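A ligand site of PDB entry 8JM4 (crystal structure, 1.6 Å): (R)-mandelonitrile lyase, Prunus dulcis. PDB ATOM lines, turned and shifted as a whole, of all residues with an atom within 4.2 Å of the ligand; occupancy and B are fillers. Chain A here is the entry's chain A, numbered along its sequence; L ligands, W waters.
Water W6 bridges O of Ala 108 (2.8 Å) and O2 of the ligand (2.8 Å). Water W7 bridges the backbone carbonyl oxygen of Gly 270 (2.8 Å) and a nitrogen (N3) of the ligand (2.9 Å). Water W8 bridges O10 of the ligand (2.9 Å) and O of His 468 (3.4 Å). Water W3 bridges NE2 of His 468 and N8 of the ligand.
The backbone NH of Thr 44 is in hydrogen-bond range of an oxygen (O1) of the ligand, at 3.1 Å. OG1 of Thr 44 sits at hydrogen-bond distance from O11 of the ligand, 2.6 Å away. O6 of the ligand is in hydrogen-bond range of OE2 of Glu 63 (2.7 Å). An oxygen (O1) of the ligand lies within hydrogen-bond range of the backbone NH of Thr 114. The side-chain hydroxyl (OG1) of Thr 114 sits at hydrogen-bond distance from an oxygen (O2) of the ligand (2.8 Å). The backbone NH (N) of Gln 508 is in hydrogen-bond range of an oxygen (O7) of the ligand, 2.8 Å away. O8 of the ligand is in hydrogen-bond range of N of Val 121 (2.9 Å). The backbone carbonyl oxygen of Val 121 sits at hydrogen-bond distance from a nitrogen (N7) of the ligand, at 2.9 Å. The backbone NH (N) of Ala 496 lies within hydrogen-bond range of an oxygen (O14) of the ligand (2.9 Å). A nitrogen (N4) of the ligand is in hydrogen-bond range of the backbone NH of Val 225 (3.0 Å). O of Val 225 lies within hydrogen-bond range of N3 of the ligand (3.0 Å). N of Arg 64 sits at hydrogen-bond distance from N5 of the ligand (3.1 Å). O6 of the ligand sits at hydrogen-bond distance from NE of Arg 64 (3.0 Å). The backbone NH of Gly 120 sits at hydrogen-bond distance from an oxygen (O8) of the ligand. The backbone NH (N) of Ala 119 sits at hydrogen-bond distance from a nitrogen (N8) of the ligand (3.1 Å). ND2 of Asn 118 lies within hydrogen-bond range of O9 of the ligand. The backbone carbonyl oxygen (O) of Ile 110 is in hydrogen-bond range of an oxygen (O5) of the ligand (3.2 Å). The backbone NH (N) of Ser 45 sits at hydrogen-bond distance from an oxygen (O13) of the ligand (3.3 Å). O6 of the ligand is in hydrogen-bond range of O of Ala 108, at 3.4 Å.
The side-chain carboxylate (OE2) of Glu 63 lies within hydrogen-bond range of the backbone NH (N) of Ile 110, at 3.3 Å. O of Val 121 sits at hydrogen-bond distance from NE2 of Gln 508, 3.1 Å away. The backbone NH of Arg 64 lies close to the backbone carbonyl oxygen of Ala 223 (3.2 Å). The guanidinium group of Arg 64 is in hydrogen-bond range of the backbone carbonyl oxygen of Ala 108 (2.9 Å). The backbone NH (N) of Gly 120 sits at hydrogen-bond distance from the side-chain amide oxygen (OD1) of Asn 118, 3.1 Å away. N of Gly 113 lies within hydrogen-bond range of O of Gly 42, at 3.4 Å. The backbone NH (N) of Gly 267 is in hydrogen-bond range of the side-chain carboxylate (OD2) of Asp 495 (2.7 Å). The backbone NH (N) of Ala 266 is in hydrogen-bond range of the backbone carbonyl oxygen (O) of Ile 40, 3.3 Å away.
An oxygen (O7) of the ligand sits close to the backbone carbonyl oxygen of His 506 (3.3 Å). An oxygen (O7) of the ligand lies close to the backbone nitrogen (N) of Pro 507 (3.0 Å). Gly 41 touches the ligand. Gly 43 touches the ligand (CA to O3, 3.4 Å). Leu 62 touches the ligand (O to C9, 3.9 Å). Val 106 touches the ligand. CA of Arg 109 touches O6 of the ligand, 3.5 Å away. Gly 113 touches the ligand (CA to O5, 3.3 Å). Ala 223 touches the ligand (O to C9, 3.3 Å). Ser 265 touches the ligand. Ala 266 touches the ligand. Gly 267 touches the ligand. Val 388 touches the ligand (CG2 to N3, 3.6 Å). Trp 467 touches the ligand (O to C20, 3.3 Å). His 468 touches the ligand (NE2 to C22, 3.3 Å). Asp 495 touches the ligand (CB to O14, 3.4 Å). Hydrophobic or aromatic side chains within 4 Å of the ligand: Val 106, Ala 119, Val 121, Val 225, Ala 266, Val 388, Trp 467, His 468, Ala 496, His 506 and Pro 507. Of the 35 residues printed, 30 come within 4 Å of the ligand. The nearest printed residue that does not touch the ligand is Ile 117 (4.01 Å).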
ATOM      1  N   ILE A  40       6.361  23.464  25.815  1.00  0.00           N
ATOM      2  CA  ILE A  40       5.178  22.773  25.218  1.00  0.00           C
ATOM      3  C   ILE A  40       3.961  23.652  25.466  1.00  0.00           C
ATOM      4  O   ILE A  40       3.506  23.734  26.668  1.00  0.00           O
ATOM      5  CB  ILE A  40       4.993  21.370  25.783  1.00  0.00           C
ATOM      6  CG1 ILE A  40       6.241  20.515  25.539  1.00  0.00           C
ATOM      7  CG2 ILE A  40       3.743  20.753  25.177  1.00  0.00           C
ATOM      8  CD1 ILE A  40       6.361  19.343  26.430  1.00  0.00           C
ATOM      9  N   GLY A  41       3.501  24.324  24.440  1.00  0.00           N
ATOM     10  CA  GLY A  41       2.341  25.188  24.625  1.00  0.00           C
ATOM     11  C   GLY A  41       2.734  26.659  24.547  1.00  0.00           C
ATOM     12  O   GLY A  41       3.265  27.206  25.571  1.00  0.00           O
ATOM     13  N   GLY A  42       2.411  27.260  23.429  1.00  0.00           N
ATOM     14  CA  GLY A  42       2.664  28.696  23.163  1.00  0.00           C
ATOM     15  C   GLY A  42       1.551  29.558  23.717  1.00  0.00           C
ATOM     16  O   GLY A  42       0.992  30.339  22.980  1.00  0.00           O
ATOM     17  N   GLY A  43       1.277  29.448  25.015  1.00  0.00           N
ATOM     18  CA  GLY A  43       0.160  30.197  25.580  1.00  0.00           C
ATOM     19  C   GLY A  43       0.601  31.280  26.543  1.00  0.00           C
ATOM     20  O   GLY A  43       1.682  31.902  26.383  1.00  0.00           O
ATOM     21  N   THR A  44      -0.179  31.483  27.602  1.00  0.00           N
ATOM     22  CA  THR A  44      -0.105  32.643  28.539  1.00  0.00           C
ATOM     23  C   THR A  44       1.216  32.605  29.276  1.00  0.00           C
ATOM     24  O   THR A  44       1.928  33.620  29.266  1.00  0.00           O
ATOM     25  CB  THR A  44      -1.289  32.629  29.512  1.00  0.00           C
ATOM     26  OG1 THR A  44      -2.460  32.580  28.673  1.00  0.00           O
ATOM     27  CG2 THR A  44      -1.314  33.840  30.435  1.00  0.00           C
ATOM     28  N   SER A  45       1.590  31.467  29.795  1.00  0.00           N
ATOM     29  CA  SER A  45       2.887  31.319  30.482  1.00  0.00           C
ATOM     30  C   SER A  45       3.955  30.943  29.441  1.00  0.00           C
ATOM     31  O   SER A  45       5.113  31.367  29.576  1.00  0.00           O
ATOM     32  CB  SER A  45       2.823  30.297  31.580  1.00  0.00           C
ATOM     33  OG  SER A  45       1.976  30.725  32.647  1.00  0.00           O
ATOM     34  N   LEU A  62       6.624  24.805  20.997  1.00  0.00           N
ATOM     35  CA  LEU A  62       5.723  23.949  20.186  1.00  0.00           C
ATOM     36  C   LEU A  62       4.294  24.324  20.537  1.00  0.00           C
ATOM     37  O   LEU A  62       3.935  24.191  21.745  1.00  0.00           O
ATOM     38  CB  LEU A  62       6.012  22.481  20.519  1.00  0.00           C
ATOM     39  CG  LEU A  62       7.394  21.992  20.113  1.00  0.00           C
ATOM     40  CD1 LEU A  62       7.662  20.620  20.673  1.00  0.00           C
ATOM     41  CD2 LEU A  62       7.548  21.992  18.600  1.00  0.00           C
ATOM     42  N   GLU A  63       3.531  24.742  19.549  1.00  0.00           N
ATOM     43  CA  GLU A  63       2.110  25.123  19.791  1.00  0.00           C
ATOM     44  C   GLU A  63       1.237  24.299  18.852  1.00  0.00           C
ATOM     45  O   GLU A  63       1.437  24.342  17.656  1.00  0.00           O
ATOM     46  CB  GLU A  63       1.927  26.625  19.632  1.00  0.00           C
ATOM     47  CG  GLU A  63       0.478  27.053  19.466  1.00  0.00           C
ATOM     48  CD  GLU A  63      -0.390  26.697  20.665  1.00  0.00           C
ATOM     49  OE1 GLU A  63       0.089  26.830  21.770  1.00  0.00           O
ATOM     50  OE2 GLU A  63      -1.538  26.272  20.451  1.00  0.00           O
ATOM     51  N   ARG A  64       0.169  23.703  19.405  1.00  0.00           N
ATOM     52  CA  ARG A  64      -0.727  22.854  18.615  1.00  0.00           C
ATOM     53  C   ARG A  64      -1.592  23.702  17.697  1.00  0.00           C
ATOM     54  O   ARG A  64      -1.977  23.219  16.620  1.00  0.00           O
ATOM     55  CB  ARG A  64      -1.549  21.955  19.536  1.00  0.00           C
ATOM     56  CG  ARG A  64      -2.638  22.728  20.246  1.00  0.00           C
ATOM     57  CD  ARG A  64      -3.428  21.874  21.251  1.00  0.00           C
ATOM     58  NE  ARG A  64      -4.428  22.741  21.889  1.00  0.00           N
ATOM     59  CZ  ARG A  64      -5.690  22.410  22.183  1.00  0.00           C
ATOM     60  NH1 ARG A  64      -6.134  21.191  21.938  1.00  0.00           N
ATOM     61  NH2 ARG A  64      -6.508  23.321  22.681  1.00  0.00           N
ATOM     62  N   VAL A 106     -14.712  26.496  27.240  1.00  0.00           N
ATOM     63  CA  VAL A 106     -13.801  26.638  26.070  1.00  0.00           C
ATOM     64  C   VAL A 106     -12.381  26.736  26.585  1.00  0.00           C
ATOM     65  O   VAL A 106     -12.160  27.230  27.723  1.00  0.00           O
ATOM     66  CB  VAL A 106     -14.077  27.855  25.158  1.00  0.00           C
ATOM     67  CG1 VAL A 106     -15.428  27.804  24.489  1.00  0.00           C
ATOM     68  CG2 VAL A 106     -13.868  29.166  25.887  1.00  0.00           C
ATOM     69  N   ALA A 108      -8.284  27.688  24.625  1.00  0.00           N
ATOM     70  CA  ALA A 108      -7.642  28.199  23.405  1.00  0.00           C
ATOM     71  C   ALA A 108      -6.863  27.109  22.653  1.00  0.00           C
ATOM     72  O   ALA A 108      -6.364  26.145  23.245  1.00  0.00           O
ATOM     73  CB  ALA A 108      -6.704  29.329  23.743  1.00  0.00           C
ATOM     74  N   ARG A 109      -6.688  27.335  21.361  1.00  0.00           N
ATOM     75  CA  ARG A 109      -5.937  26.456  20.460  1.00  0.00           C
ATOM     76  C   ARG A 109      -5.274  27.365  19.438  1.00  0.00           C
ATOM     77  O   ARG A 109      -5.769  27.457  18.328  1.00  0.00           O
ATOM     78  CB  ARG A 109      -6.889  25.444  19.807  1.00  0.00           C
ATOM     79  CG  ARG A 109      -6.176  24.428  18.924  1.00  0.00           C
ATOM     80  CD  ARG A 109      -7.025  23.228  18.488  1.00  0.00           C
ATOM     81  NE  ARG A 109      -8.263  23.717  18.035  1.00  0.00           N
ATOM     82  CZ  ARG A 109      -9.487  23.224  18.165  1.00  0.00           C
ATOM     83  NH1 ARG A 109      -9.839  22.118  18.826  1.00  0.00           N
ATOM     84  NH2 ARG A 109     -10.425  23.990  17.673  1.00  0.00           N
ATOM     85  N   ILE A 110      -4.238  28.079  19.866  1.00  0.00           N
ATOM     86  CA  ILE A 110      -3.743  29.207  19.020  1.00  0.00           C
ATOM     87  C   ILE A 110      -2.457  29.725  19.623  1.00  0.00           C
ATOM     88  O   ILE A 110      -2.267  29.658  20.837  1.00  0.00           O
ATOM     89  CB  ILE A 110      -4.812  30.328  18.910  1.00  0.00           C
ATOM     90  CG1 ILE A 110      -4.575  31.203  17.684  1.00  0.00           C
ATOM     91  CG2 ILE A 110      -4.803  31.133  20.217  1.00  0.00           C
ATOM     92  CD1 ILE A 110      -4.839  30.565  16.313  1.00  0.00           C
ATOM     93  N   GLY A 113      -2.226  31.416  23.049  1.00  0.00           N
ATOM     94  CA  GLY A 113      -3.103  30.740  23.990  1.00  0.00           C
ATOM     95  C   GLY A 113      -4.294  31.564  24.374  1.00  0.00           C
ATOM     96  O   GLY A 113      -4.948  32.173  23.487  1.00  0.00           O
ATOM     97  N   THR A 114      -4.704  31.461  25.615  1.00  0.00           N
ATOM     98  CA  THR A 114      -6.021  31.983  25.998  1.00  0.00           C
ATOM     99  C   THR A 114      -5.996  33.524  25.954  1.00  0.00           C
ATOM    100  O   THR A 114      -7.047  34.092  25.775  1.00  0.00           O
ATOM    101  CB  THR A 114      -6.464  31.340  27.315  1.00  0.00           C
ATOM    102  OG1 THR A 114      -6.537  29.950  27.007  1.00  0.00           O
ATOM    103  CG2 THR A 114      -7.820  31.818  27.785  1.00  0.00           C
ATOM    104  N   ILE A 117      -8.037  34.891  23.039  1.00  0.00           N
ATOM    105  CA  ILE A 117      -9.517  34.709  22.951  1.00  0.00           C
ATOM    106  C   ILE A 117     -10.261  35.243  24.180  1.00  0.00           C
ATOM    107  O   ILE A 117     -11.463  35.068  24.247  1.00  0.00           O
ATOM    108  CB  ILE A 117      -9.863  33.217  22.743  1.00  0.00           C
ATOM    109  CG1 ILE A 117      -9.392  32.357  23.914  1.00  0.00           C
ATOM    110  CG2 ILE A 117      -9.358  32.684  21.403  1.00  0.00           C
ATOM    111  CD1 ILE A 117     -10.152  30.999  24.065  1.00  0.00           C
ATOM    112  N   ASN A 118      -9.556  35.835  25.144  1.00  0.00           N
ATOM    113  CA  ASN A 118     -10.106  36.110  26.472  1.00  0.00           C
ATOM    114  C   ASN A 118     -10.710  37.525  26.514  1.00  0.00           C
ATOM    115  O   ASN A 118     -10.739  38.261  25.460  1.00  0.00           O
ATOM    116  CB  ASN A 118      -9.071  35.828  27.582  1.00  0.00           C
ATOM    117  CG  ASN A 118      -7.958  36.839  27.701  1.00  0.00           C
ATOM    118  OD1 ASN A 118      -7.962  37.899  27.068  1.00  0.00           O
ATOM    119  ND2 ASN A 118      -6.959  36.485  28.495  1.00  0.00           N
ATOM    120  N   ALA A 119     -11.171  37.922  27.680  1.00  0.00           N
ATOM    121  CA  ALA A 119     -11.957  39.158  27.864  1.00  0.00           C
ATOM    122  C   ALA A 119     -11.042  40.334  28.208  1.00  0.00           C
ATOM    123  O   ALA A 119     -11.565  41.465  28.407  1.00  0.00           O
ATOM    124  CB  ALA A 119     -13.055  38.923  28.862  1.00  0.00           C
ATOM    125  N   GLY A 120      -9.713  40.146  28.184  1.00  0.00           N
ATOM    126  CA  GLY A 120      -8.740  41.228  28.184  1.00  0.00           C
ATOM    127  C   GLY A 120      -8.448  41.810  29.550  1.00  0.00           C
ATOM    128  O   GLY A 120      -7.656  42.712  29.673  1.00  0.00           O
ATOM    129  N   VAL A 121      -9.168  41.396  30.587  1.00  0.00           N
ATOM    130  CA  VAL A 121      -9.013  42.108  31.884  1.00  0.00           C
ATOM    131  C   VAL A 121      -7.640  41.804  32.461  1.00  0.00           C
ATOM    132  O   VAL A 121      -7.277  40.604  32.587  1.00  0.00           O
ATOM    133  CB  VAL A 121     -10.073  41.667  32.900  1.00  0.00           C
ATOM    134  CG1 VAL A 121      -9.931  42.409  34.215  1.00  0.00           C
ATOM    135  CG2 VAL A 121     -11.474  41.753  32.333  1.00  0.00           C
ATOM    136  N   ALA A 223       1.867  22.105  15.883  1.00  0.00           N
ATOM    137  CA  ALA A 223       2.752  21.103  16.513  1.00  0.00           C
ATOM    138  C   ALA A 223       1.983  20.468  17.669  1.00  0.00           C
ATOM    139  O   ALA A 223       1.920  21.098  18.769  1.00  0.00           O
ATOM    140  CB  ALA A 223       4.050  21.720  17.025  1.00  0.00           C
ATOM    141  N   SER A 224       1.414  19.274  17.479  1.00  0.00           N
ATOM    142  CA  SER A 224       0.624  18.599  18.532  1.00  0.00           C
ATOM    143  C   SER A 224       1.578  17.702  19.310  1.00  0.00           C
ATOM    144  O   SER A 224       2.012  16.642  18.757  1.00  0.00           O
ATOM    145  CB  SER A 224      -0.565  17.852  17.905  1.00  0.00           C
ATOM    146  OG  SER A 224      -1.175  16.999  18.852  1.00  0.00           O
ATOM    147  N   VAL A 225       1.966  18.113  20.509  1.00  0.00           N
ATOM    148  CA  VAL A 225       2.952  17.367  21.339  1.00  0.00           C
ATOM    149  C   VAL A 225       2.242  16.187  21.997  1.00  0.00           C
ATOM    150  O   VAL A 225       1.291  16.395  22.763  1.00  0.00           O
ATOM    151  CB  VAL A 225       3.635  18.227  22.395  1.00  0.00           C
ATOM    152  CG1 VAL A 225       4.611  17.355  23.145  1.00  0.00           C
ATOM    153  CG2 VAL A 225       4.329  19.396  21.735  1.00  0.00           C
ATOM    154  N   SER A 265       3.666  23.805  29.377  1.00  0.00           N
ATOM    155  CA  SER A 265       2.893  25.046  29.522  1.00  0.00           C
ATOM    156  C   SER A 265       1.591  24.881  28.730  1.00  0.00           C
ATOM    157  O   SER A 265       1.141  25.809  28.044  1.00  0.00           O
ATOM    158  CB  SER A 265       3.701  26.247  29.087  1.00  0.00           C
ATOM    159  OG  SER A 265       4.900  26.399  29.877  1.00  0.00           O
ATOM    160  N   ALA A 266       1.024  23.680  28.802  1.00  0.00           N
ATOM    161  CA  ALA A 266      -0.114  23.254  27.934  1.00  0.00           C
ATOM    162  C   ALA A 266      -1.468  23.567  28.588  1.00  0.00           C
ATOM    163  O   ALA A 266      -2.490  23.194  28.005  1.00  0.00           O
ATOM    164  CB  ALA A 266       0.006  21.777  27.591  1.00  0.00           C
ATOM    165  N   GLY A 267      -1.493  24.220  29.753  1.00  0.00           N
ATOM    166  CA  GLY A 267      -2.715  24.669  30.441  1.00  0.00           C
ATOM    167  C   GLY A 267      -3.252  23.648  31.410  1.00  0.00           C
ATOM    168  O   GLY A 267      -2.726  22.510  31.464  1.00  0.00           O
ATOM    169  N   GLY A 270      -4.274  20.696  29.128  1.00  0.00           N
ATOM    170  CA  GLY A 270      -3.279  20.038  28.275  1.00  0.00           C
ATOM    171  C   GLY A 270      -2.107  19.500  29.073  1.00  0.00           C
ATOM    172  O   GLY A 270      -1.483  18.490  28.623  1.00  0.00           O
ATOM    173  N   VAL A 388      -3.467  12.688  21.587  1.00  0.00           N
ATOM    174  CA  VAL A 388      -3.505  13.973  22.366  1.00  0.00           C
ATOM    175  C   VAL A 388      -4.565  14.901  21.776  1.00  0.00           C
ATOM    176  O   VAL A 388      -4.986  15.822  22.454  1.00  0.00           O
ATOM    177  CB  VAL A 388      -2.120  14.641  22.424  1.00  0.00           C
ATOM    178  CG1 VAL A 388      -1.743  15.308  21.088  1.00  0.00           C
ATOM    179  CG2 VAL A 388      -2.042  15.593  23.586  1.00  0.00           C
ATOM    180  N   TRP A 467     -14.354  30.660  33.399  1.00  0.00           N
ATOM    181  CA  TRP A 467     -13.257  30.437  32.430  1.00  0.00           C
ATOM    182  C   TRP A 467     -11.896  30.521  33.120  1.00  0.00           C
ATOM    183  O   TRP A 467     -10.883  30.475  32.399  1.00  0.00           O
ATOM    184  CB  TRP A 467     -13.340  31.460  31.293  1.00  0.00           C
ATOM    185  CG  TRP A 467     -14.594  31.438  30.464  1.00  0.00           C
ATOM    186  CD1 TRP A 467     -15.192  30.357  29.895  1.00  0.00           C
ATOM    187  CD2 TRP A 467     -15.345  32.568  30.010  1.00  0.00           C
ATOM    188  NE1 TRP A 467     -16.257  30.713  29.113  1.00  0.00           N
ATOM    189  CE2 TRP A 467     -16.383  32.070  29.175  1.00  0.00           C
ATOM    190  CE3 TRP A 467     -15.246  33.955  30.220  1.00  0.00           C
ATOM    191  CZ2 TRP A 467     -17.307  32.920  28.563  1.00  0.00           C
ATOM    192  CZ3 TRP A 467     -16.149  34.780  29.580  1.00  0.00           C
ATOM    193  CH2 TRP A 467     -17.156  34.270  28.770  1.00  0.00           C
ATOM    194  N   HIS A 468     -11.842  30.676  34.424  1.00  0.00           N
ATOM    195  CA  HIS A 468     -10.571  30.860  35.141  1.00  0.00           C
ATOM    196  C   HIS A 468     -10.126  29.554  35.813  1.00  0.00           C
ATOM    197  O   HIS A 468      -9.657  29.595  36.948  1.00  0.00           O
ATOM    198  CB  HIS A 468     -10.649  32.001  36.120  1.00  0.00           C
ATOM    199  CG  HIS A 468     -10.914  33.329  35.480  1.00  0.00           C
ATOM    200  ND1 HIS A 468     -10.971  34.474  36.239  1.00  0.00           N
ATOM    201  CD2 HIS A 468     -11.148  33.718  34.205  1.00  0.00           C
ATOM    202  CE1 HIS A 468     -11.180  35.516  35.439  1.00  0.00           C
ATOM    203  NE2 HIS A 468     -11.331  35.076  34.209  1.00  0.00           N
ATOM    204  N   ASP A 495       2.193  27.106  34.036  1.00  0.00           N
ATOM    205  CA  ASP A 495       0.900  27.504  33.457  1.00  0.00           C
ATOM    206  C   ASP A 495      -0.130  27.459  34.601  1.00  0.00           C
ATOM    207  O   ASP A 495       0.266  27.290  35.771  1.00  0.00           O
ATOM    208  CB  ASP A 495       0.452  26.630  32.288  1.00  0.00           C
ATOM    209  CG  ASP A 495       0.337  25.152  32.612  1.00  0.00           C
ATOM    210  OD1 ASP A 495       0.187  24.858  33.788  1.00  0.00           O
ATOM    211  OD2 ASP A 495       0.454  24.313  31.633  1.00  0.00           O
ATOM    212  N   ALA A 496      -1.406  27.590  34.300  1.00  0.00           N
ATOM    213  CA  ALA A 496      -2.458  27.641  35.329  1.00  0.00           C
ATOM    214  C   ALA A 496      -2.749  26.276  35.931  1.00  0.00           C
ATOM    215  O   ALA A 496      -3.567  26.213  36.859  1.00  0.00           O
ATOM    216  CB  ALA A 496      -3.697  28.282  34.782  1.00  0.00           C
ATOM    217  N   HIS A 506      -8.757  37.882  38.014  1.00  0.00           N
ATOM    218  CA  HIS A 506      -8.459  37.832  36.561  1.00  0.00           C
ATOM    219  C   HIS A 506      -6.988  37.436  36.416  1.00  0.00           C
ATOM    220  O   HIS A 506      -6.110  38.274  36.641  1.00  0.00           O
ATOM    221  CB  HIS A 506      -8.810  39.159  35.920  1.00  0.00           C
ATOM    222  CG  HIS A 506     -10.265  39.396  35.848  1.00  0.00           C
ATOM    223  ND1 HIS A 506     -10.971  39.938  36.910  1.00  0.00           N
ATOM    224  CD2 HIS A 506     -11.173  39.092  34.905  1.00  0.00           C
ATOM    225  CE1 HIS A 506     -12.249  39.990  36.591  1.00  0.00           C
ATOM    226  NE2 HIS A 506     -12.414  39.452  35.351  1.00  0.00           N
ATOM    227  N   PRO A 507      -6.699  36.133  36.202  1.00  0.00           N
ATOM    228  CA  PRO A 507      -5.361  35.629  36.416  1.00  0.00           C
ATOM    229  C   PRO A 507      -4.373  35.716  35.256  1.00  0.00           C
ATOM    230  O   PRO A 507      -3.255  35.323  35.461  1.00  0.00           O
ATOM    231  CB  PRO A 507      -5.701  34.164  36.772  1.00  0.00           C
ATOM    232  CG  PRO A 507      -6.852  33.832  35.830  1.00  0.00           C
ATOM    233  CD  PRO A 507      -7.701  35.078  35.956  1.00  0.00           C
ATOM    234  N   GLN A 508      -4.774  36.194  34.100  1.00  0.00           N
ATOM    235  CA  GLN A 508      -3.846  36.225  32.944  1.00  0.00           C
ATOM    236  C   GLN A 508      -2.594  37.007  33.337  1.00  0.00           C
ATOM    237  O   GLN A 508      -1.491  36.546  33.007  1.00  0.00           O
ATOM    238  CB  GLN A 508      -4.502  36.728  31.665  1.00  0.00           C
ATOM    239  CG  GLN A 508      -4.716  38.227  31.573  1.00  0.00           C
ATOM    240  CD  GLN A 508      -4.975  38.719  30.162  1.00  0.00           C
ATOM    241  OE1 GLN A 508      -4.556  38.113  29.186  1.00  0.00           O
ATOM    242  NE2 GLN A 508      -5.642  39.887  30.060  1.00  0.00           N
HETATM  243  P1  LIG L   1      -3.197  28.724  27.732  1.00  0.00           P
HETATM  244  O1  LIG L   1      -2.996  30.196  27.580  1.00  0.00           O
HETATM  245  O2  LIG L   1      -4.462  28.152  27.183  1.00  0.00           O
HETATM  246  O3  LIG L   1      -1.945  28.026  27.072  1.00  0.00           O
HETATM  247  C1  LIG L   1      -1.875  26.593  26.783  1.00  0.00           C
HETATM  248  C2  LIG L   1      -1.431  26.427  25.349  1.00  0.00           C
HETATM  249  O4  LIG L   1      -0.996  25.045  25.134  1.00  0.00           O
HETATM  250  C3  LIG L   1      -2.507  26.736  24.304  1.00  0.00           C
HETATM  251  O5  LIG L   1      -2.066  27.700  23.344  1.00  0.00           O
HETATM  252  C4  LIG L   1      -2.753  25.358  23.673  1.00  0.00           C
HETATM  253  O6  LIG L   1      -3.190  25.419  22.348  1.00  0.00           O
HETATM  254  C5  LIG L   1      -1.421  24.647  23.849  1.00  0.00           C
HETATM  255  N1  LIG L   1      -1.433  23.189  23.893  1.00  0.00           N
HETATM  256  C6  LIG L   1      -2.226  22.386  24.696  1.00  0.00           C
HETATM  257  N2  LIG L   1      -1.900  21.128  24.647  1.00  0.00           N
HETATM  258  C7  LIG L   1      -0.851  21.098  23.718  1.00  0.00           C
HETATM  259  C8  LIG L   1      -0.089  20.031  23.186  1.00  0.00           C
HETATM  260  N3  LIG L   1      -0.280  18.779  23.587  1.00  0.00           N
HETATM  261  N4  LIG L   1       0.880  20.343  22.282  1.00  0.00           N
HETATM  262  C9  LIG L   1       1.029  21.630  21.915  1.00  0.00           C
HETATM  263  N5  LIG L   1       0.395  22.720  22.373  1.00  0.00           N
HETATM  264  C10 LIG L   1      -0.551  22.362  23.270  1.00  0.00           C
HETATM  265  N6  LIG L   1      -8.253  35.846  32.620  1.00  0.00           N
HETATM  266  C11 LIG L   1      -8.001  37.181  32.809  1.00  0.00           C
HETATM  267  O7  LIG L   1      -7.150  37.551  33.603  1.00  0.00           O
HETATM  268  N7  LIG L   1      -8.755  38.141  32.176  1.00  0.00           N
HETATM  269  C12 LIG L   1      -9.837  37.849  31.372  1.00  0.00           C
HETATM  270  O8  LIG L   1     -10.452  38.795  30.817  1.00  0.00           O
HETATM  271  C13 LIG L   1     -10.057  36.489  31.067  1.00  0.00           C
HETATM  272  N8  LIG L   1     -11.028  36.187  30.227  1.00  0.00           N
HETATM  273  C14 LIG L   1     -11.100  34.876  29.837  1.00  0.00           C
HETATM  274  C15 LIG L   1     -12.028  34.539  28.842  1.00  0.00           C
HETATM  275  C16 LIG L   1     -12.121  33.274  28.329  1.00  0.00           C
HETATM  276  C17 LIG L   1     -13.113  32.955  27.234  1.00  0.00           C
HETATM  277  C18 LIG L   1     -11.278  32.279  28.842  1.00  0.00           C
HETATM  278  C19 LIG L   1     -11.341  30.873  28.325  1.00  0.00           C
HETATM  279  C20 LIG L   1     -10.402  32.559  29.903  1.00  0.00           C
HETATM  280  C21 LIG L   1     -10.272  33.861  30.390  1.00  0.00           C
HETATM  281  N9  LIG L   1      -9.357  34.214  31.393  1.00  0.00           N
HETATM  282  C22 LIG L   1      -9.177  35.524  31.726  1.00  0.00           C
HETATM  283  C23 LIG L   1      -8.479  33.192  32.003  1.00  0.00           C
HETATM  284  C24 LIG L   1      -7.037  33.302  31.554  1.00  0.00           C
HETATM  285  O9  LIG L   1      -7.009  33.858  30.288  1.00  0.00           O
HETATM  286  C25 LIG L   1      -6.446  31.896  31.570  1.00  0.00           C
HETATM  287  O10 LIG L   1      -6.666  31.277  32.854  1.00  0.00           O
HETATM  288  C26 LIG L   1      -4.961  31.835  31.210  1.00  0.00           C
HETATM  289  O11 LIG L   1      -4.760  32.478  29.934  1.00  0.00           O
HETATM  290  C27 LIG L   1      -4.500  30.398  31.130  1.00  0.00           C
HETATM  291  O12 LIG L   1      -3.065  30.395  30.722  1.00  0.00           O
HETATM  292  P2  LIG L   1      -2.282  29.002  30.480  1.00  0.00           P
HETATM  293  O13 LIG L   1      -0.907  29.344  29.998  1.00  0.00           O
HETATM  294  O14 LIG L   1      -2.524  28.093  31.645  1.00  0.00           O
HETATM  295  O15 LIG L   1      -3.141  28.384  29.286  1.00  0.00           O
HETATM  296  O   HOH W   1      -4.997  26.890  31.684  1.00  0.00           O
HETATM  297  O   HOH W   2      -7.134  28.609  32.711  1.00  0.00           O
HETATM  298  O   HOH W   3     -13.233  36.720  32.586  1.00  0.00           O
HETATM  299  O   HOH W   4      -5.182  39.645  34.534  1.00  0.00           O
HETATM  300  O   HOH W   5      -4.117  19.291  24.688  1.00  0.00           O
HETATM  301  O   HOH W   6      -5.583  25.915  25.874  1.00  0.00           O
HETATM  302  O   HOH W   7      -1.719  17.865  25.894  1.00  0.00           O
HETATM  303  O   HOH W   8      -6.640  30.424  35.623  1.00  0.00           O
HETATM  304  O   HOH W   9       1.139  28.534  28.218  1.00  0.00           O
HETATM  305  O   HOH W  10      -6.062  26.848  29.266  1.00  0.00           O
